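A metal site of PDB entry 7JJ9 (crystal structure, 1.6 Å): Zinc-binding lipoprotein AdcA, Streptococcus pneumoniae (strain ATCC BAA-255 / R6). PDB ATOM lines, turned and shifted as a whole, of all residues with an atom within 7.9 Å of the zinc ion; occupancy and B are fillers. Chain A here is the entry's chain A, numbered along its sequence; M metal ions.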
ATOM      1  N   PHE A   9      -7.394  -9.199  -3.992  1.00  0.00           N
ATOM      2  CA  PHE A   9      -7.376 -10.640  -3.879  1.00  0.00           C
ATOM      3  C   PHE A   9      -8.755 -11.169  -3.491  1.00  0.00           C
ATOM      4  O   PHE A   9      -9.723 -10.415  -3.324  1.00  0.00           O
ATOM      5  CB  PHE A   9      -6.257 -11.095  -2.923  1.00  0.00           C
ATOM      6  CG  PHE A   9      -6.498 -10.766  -1.467  1.00  0.00           C
ATOM      7  CD1 PHE A   9      -6.414  -9.466  -1.015  1.00  0.00           C
ATOM      8  CD2 PHE A   9      -6.805 -11.769  -0.540  1.00  0.00           C
ATOM      9  CE1 PHE A   9      -6.672  -9.160   0.314  1.00  0.00           C
ATOM     10  CE2 PHE A   9      -7.065 -11.475   0.773  1.00  0.00           C
ATOM     11  CZ  PHE A   9      -7.003 -10.169   1.224  1.00  0.00           C
ATOM     12  N   PRO A  36      -1.212 -13.868  -1.960  1.00  0.00           N
ATOM     13  CA  PRO A  36      -1.433 -12.422  -1.881  1.00  0.00           C
ATOM     14  C   PRO A  36      -0.508 -11.668  -0.944  1.00  0.00           C
ATOM     15  O   PRO A  36      -0.220 -10.490  -1.188  1.00  0.00           O
ATOM     16  CB  PRO A  36      -2.902 -12.316  -1.409  1.00  0.00           C
ATOM     17  CG  PRO A  36      -3.518 -13.589  -1.967  1.00  0.00           C
ATOM     18  CD  PRO A  36      -2.456 -14.627  -1.739  1.00  0.00           C
ATOM     19  N   HIS A  37      -0.042 -12.292   0.124  1.00  0.00           N
ATOM     20  CA  HIS A  37       0.892 -11.605   1.008  1.00  0.00           C
ATOM     21  C   HIS A  37       2.216 -11.306   0.321  1.00  0.00           C
ATOM     22  O   HIS A  37       2.941 -10.417   0.794  1.00  0.00           O
ATOM     23  CB  HIS A  37       1.204 -12.412   2.255  1.00  0.00           C
ATOM     24  CG  HIS A  37       0.057 -12.551   3.223  1.00  0.00           C
ATOM     25  ND1 HIS A  37      -0.345 -11.532   4.047  1.00  0.00           N
ATOM     26  CD2 HIS A  37      -0.712 -13.621   3.542  1.00  0.00           C
ATOM     27  CE1 HIS A  37      -1.346 -11.958   4.812  1.00  0.00           C
ATOM     28  NE2 HIS A  37      -1.568 -13.229   4.541  1.00  0.00           N
ATOM     29  N   MET A  62      -2.602  -5.543   4.927  1.00  0.00           N
ATOM     30  CA  MET A  62      -2.608  -6.732   4.065  1.00  0.00           C
ATOM     31  C   MET A  62      -1.859  -6.409   2.796  1.00  0.00           C
ATOM     32  O   MET A  62      -0.751  -6.927   2.562  1.00  0.00           O
ATOM     33  CB  MET A  62      -4.047  -7.174   3.761  1.00  0.00           C
ATOM     34  CG  MET A  62      -4.189  -8.345   2.784  1.00  0.00           C
ATOM     35  SD  MET A  62      -3.518  -9.826   3.528  1.00  0.00           S
ATOM     36  CE  MET A  62      -3.405 -10.878   2.098  1.00  0.00           C
ATOM     37  N   ASP A 112      -2.859  -7.068  12.376  1.00  0.00           N
ATOM     38  CA  ASP A 112      -3.302  -8.310  11.739  1.00  0.00           C
ATOM     39  C   ASP A 112      -4.505  -7.978  10.864  1.00  0.00           C
ATOM     40  O   ASP A 112      -5.521  -7.477  11.376  1.00  0.00           O
ATOM     41  CB  ASP A 112      -3.641  -9.317  12.831  1.00  0.00           C
ATOM     42  CG  ASP A 112      -4.257 -10.591  12.311  1.00  0.00           C
ATOM     43  OD1 ASP A 112      -4.455 -10.711  11.086  1.00  0.00           O
ATOM     44  OD2 ASP A 112      -4.608 -11.444  13.167  1.00  0.00           O
ATOM     45  N   PRO A 113      -4.431  -8.182   9.539  1.00  0.00           N
ATOM     46  CA  PRO A 113      -5.517  -7.754   8.658  1.00  0.00           C
ATOM     47  C   PRO A 113      -6.667  -8.739   8.510  1.00  0.00           C
ATOM     48  O   PRO A 113      -7.652  -8.401   7.844  1.00  0.00           O
ATOM     49  CB  PRO A 113      -4.804  -7.579   7.311  1.00  0.00           C
ATOM     50  CG  PRO A 113      -3.772  -8.688   7.324  1.00  0.00           C
ATOM     51  CD  PRO A 113      -3.252  -8.629   8.753  1.00  0.00           C
ATOM     52  N   HIS A 114      -6.561  -9.936   9.065  1.00  0.00           N
ATOM     53  CA  HIS A 114      -7.378 -11.072   8.636  1.00  0.00           C
ATOM     54  C   HIS A 114      -8.817 -11.050   9.172  1.00  0.00           C
ATOM     55  O   HIS A 114      -9.354 -12.100   9.556  1.00  0.00           O
ATOM     56  CB  HIS A 114      -6.684 -12.372   9.051  1.00  0.00           C
ATOM     57  CG  HIS A 114      -5.416 -12.684   8.296  1.00  0.00           C
ATOM     58  ND1 HIS A 114      -4.159 -12.446   8.819  1.00  0.00           N
ATOM     59  CD2 HIS A 114      -5.218 -13.291   7.103  1.00  0.00           C
ATOM     60  CE1 HIS A 114      -3.246 -12.882   7.975  1.00  0.00           C
ATOM     61  NE2 HIS A 114      -3.865 -13.398   6.925  1.00  0.00           N
ATOM     62  N   TRP A 116     -11.624 -10.915   7.670  1.00  0.00           N
ATOM     63  CA  TRP A 116     -12.682 -11.515   6.854  1.00  0.00           C
ATOM     64  C   TRP A 116     -12.911 -13.001   7.162  1.00  0.00           C
ATOM     65  O   TRP A 116     -13.862 -13.573   6.629  1.00  0.00           O
ATOM     66  CB  TRP A 116     -12.405 -11.333   5.354  1.00  0.00           C
ATOM     67  CG  TRP A 116     -11.195 -12.097   4.848  1.00  0.00           C
ATOM     68  CD1 TRP A 116     -11.186 -13.372   4.368  1.00  0.00           C
ATOM     69  CD2 TRP A 116      -9.813 -11.669   4.865  1.00  0.00           C
ATOM     70  NE1 TRP A 116      -9.907 -13.766   4.065  1.00  0.00           N
ATOM     71  CE2 TRP A 116      -9.042 -12.754   4.389  1.00  0.00           C
ATOM     72  CE3 TRP A 116      -9.163 -10.502   5.235  1.00  0.00           C
ATOM     73  CZ2 TRP A 116      -7.648 -12.676   4.251  1.00  0.00           C
ATOM     74  CZ3 TRP A 116      -7.795 -10.437   5.110  1.00  0.00           C
ATOM     75  CH2 TRP A 116      -7.058 -11.511   4.630  1.00  0.00           C
ATOM     76  N   LEU A 117     -12.086 -13.635   7.986  1.00  0.00           N
ATOM     77  CA  LEU A 117     -12.322 -15.020   8.421  1.00  0.00           C
ATOM     78  C   LEU A 117     -13.302 -15.112   9.591  1.00  0.00           C
ATOM     79  O   LEU A 117     -13.518 -16.212  10.099  1.00  0.00           O
ATOM     80  CB  LEU A 117     -11.003 -15.692   8.807  1.00  0.00           C
ATOM     81  CG  LEU A 117     -10.083 -16.116   7.664  1.00  0.00           C
ATOM     82  CD1 LEU A 117     -10.836 -16.833   6.560  1.00  0.00           C
ATOM     83  CD2 LEU A 117      -9.301 -14.925   7.142  1.00  0.00           C
ATOM     84  N   HIS A 178      -0.955 -20.915   9.096  1.00  0.00           N
ATOM     85  CA  HIS A 178      -1.256 -19.562   8.619  1.00  0.00           C
ATOM     86  C   HIS A 178      -2.129 -18.890   9.663  1.00  0.00           C
ATOM     87  O   HIS A 178      -3.268 -19.321   9.906  1.00  0.00           O
ATOM     88  CB  HIS A 178      -1.945 -19.635   7.258  1.00  0.00           C
ATOM     89  CG  HIS A 178      -2.026 -18.343   6.527  1.00  0.00           C
ATOM     90  ND1 HIS A 178      -1.718 -18.237   5.183  1.00  0.00           N
ATOM     91  CD2 HIS A 178      -2.481 -17.123   6.897  1.00  0.00           C
ATOM     92  CE1 HIS A 178      -1.930 -16.993   4.779  1.00  0.00           C
ATOM     93  NE2 HIS A 178      -2.360 -16.290   5.817  1.00  0.00           N
ATOM     94  N   ALA A 179      -1.635 -17.796  10.235  1.00  0.00           N
ATOM     95  CA  ALA A 179      -2.291 -17.151  11.377  1.00  0.00           C
ATOM     96  C   ALA A 179      -3.357 -16.169  10.922  1.00  0.00           C
ATOM     97  O   ALA A 179      -3.289 -14.969  11.200  1.00  0.00           O
ATOM     98  CB  ALA A 179      -1.249 -16.454  12.239  1.00  0.00           C
ATOM     99  N   ALA A 180      -4.377 -16.691  10.230  1.00  0.00           N
ATOM    100  CA  ALA A 180      -5.452 -15.882   9.661  1.00  0.00           C
ATOM    101  C   ALA A 180      -6.728 -15.908  10.486  1.00  0.00           C
ATOM    102  O   ALA A 180      -7.753 -15.379  10.049  1.00  0.00           O
ATOM    103  CB  ALA A 180      -5.751 -16.350   8.246  1.00  0.00           C
ATOM    104  N   PHE A 181      -6.713 -16.556  11.654  1.00  0.00           N
ATOM    105  CA  PHE A 181      -7.955 -16.962  12.304  1.00  0.00           C
ATOM    106  C   PHE A 181      -8.088 -16.379  13.699  1.00  0.00           C
ATOM    107  O   PHE A 181      -8.903 -16.871  14.496  1.00  0.00           O
ATOM    108  CB  PHE A 181      -8.035 -18.483  12.302  1.00  0.00           C
ATOM    109  CG  PHE A 181      -7.915 -19.039  10.917  1.00  0.00           C
ATOM    110  CD1 PHE A 181      -8.987 -18.965  10.051  1.00  0.00           C
ATOM    111  CD2 PHE A 181      -6.700 -19.508  10.430  1.00  0.00           C
ATOM    112  CE1 PHE A 181      -8.872 -19.417   8.718  1.00  0.00           C
ATOM    113  CE2 PHE A 181      -6.571 -19.957   9.153  1.00  0.00           C
ATOM    114  CZ  PHE A 181      -7.673 -19.912   8.275  1.00  0.00           C
ATOM    115  N   GLU A 227      -2.877 -23.814   5.271  1.00  0.00           N
ATOM    116  CA  GLU A 227      -3.669 -22.903   4.440  1.00  0.00           C
ATOM    117  C   GLU A 227      -4.230 -23.609   3.194  1.00  0.00           C
ATOM    118  O   GLU A 227      -5.246 -23.176   2.639  1.00  0.00           O
ATOM    119  CB  GLU A 227      -2.802 -21.711   4.051  1.00  0.00           C
ATOM    120  CG  GLU A 227      -1.597 -22.125   3.226  1.00  0.00           C
ATOM    121  CD  GLU A 227      -0.673 -20.998   2.898  1.00  0.00           C
ATOM    122  OE1 GLU A 227      -0.218 -20.939   1.735  1.00  0.00           O
ATOM    123  OE2 GLU A 227      -0.379 -20.181   3.778  1.00  0.00           O
ATOM    124  N   PRO A 251      -7.466 -19.712   4.510  1.00  0.00           N
ATOM    125  CA  PRO A 251      -7.660 -18.286   4.817  1.00  0.00           C
ATOM    126  C   PRO A 251      -8.454 -17.552   3.766  1.00  0.00           C
ATOM    127  O   PRO A 251      -8.592 -16.326   3.860  1.00  0.00           O
ATOM    128  CB  PRO A 251      -6.228 -17.776   4.882  1.00  0.00           C
ATOM    129  CG  PRO A 251      -5.493 -18.588   3.902  1.00  0.00           C
ATOM    130  CD  PRO A 251      -6.088 -20.000   4.051  1.00  0.00           C
ATOM    131  N   LEU A 252      -8.922 -18.233   2.745  1.00  0.00           N
ATOM    132  CA  LEU A 252      -9.775 -17.633   1.743  1.00  0.00           C
ATOM    133  C   LEU A 252      -9.082 -16.460   1.063  1.00  0.00           C
ATOM    134  O   LEU A 252      -9.704 -15.449   0.735  1.00  0.00           O
ATOM    135  CB  LEU A 252     -11.094 -17.209   2.370  1.00  0.00           C
ATOM    136  CG  LEU A 252     -11.964 -16.714   1.269  1.00  0.00           C
ATOM    137  CD1 LEU A 252     -13.102 -17.561   1.137  1.00  0.00           C
ATOM    138  CD2 LEU A 252     -12.278 -15.272   1.606  1.00  0.00           C
ATOM    139  N   GLU A 253      -7.787 -16.611   0.826  1.00  0.00           N
ATOM    140  CA  GLU A 253      -7.010 -15.598   0.120  1.00  0.00           C
ATOM    141  C   GLU A 253      -6.877 -15.882  -1.365  1.00  0.00           C
ATOM    142  O   GLU A 253      -6.656 -14.947  -2.139  1.00  0.00           O
ATOM    143  CB  GLU A 253      -5.623 -15.471   0.750  1.00  0.00           C
ATOM    144  CG  GLU A 253      -5.723 -14.921   2.173  1.00  0.00           C
ATOM    145  CD  GLU A 253      -4.463 -14.961   3.015  1.00  0.00           C
ATOM    146  OE1 GLU A 253      -3.379 -15.415   2.560  1.00  0.00           O
ATOM    147  OE2 GLU A 253      -4.596 -14.517   4.187  1.00  0.00           O
HETATM  148 ZN    ZN M   1      -3.007 -14.367   5.355  1.00  0.00          ZN
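Within 4 Å of the zinc ion: His 37, His 114, His 178 and Glu 253.
ND1 of His 178 is in hydrogen-bond range of OE2 of Glu 227, at 2.7 Å.
SD of Met 62 sits close to ND1 of His 37 (3.6 Å).
A ring nitrogen (ND1) of His 114 sits at hydrogen-bond distance from the side-chain carboxylate of Asp 112 (2.9 Å).
The zinc ion is bound by OE2 of Glu 253, NE2 of His 37, NE2 of His 114 and NE2 of His 178.
The zinc ion has four donor atoms within binding distance.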
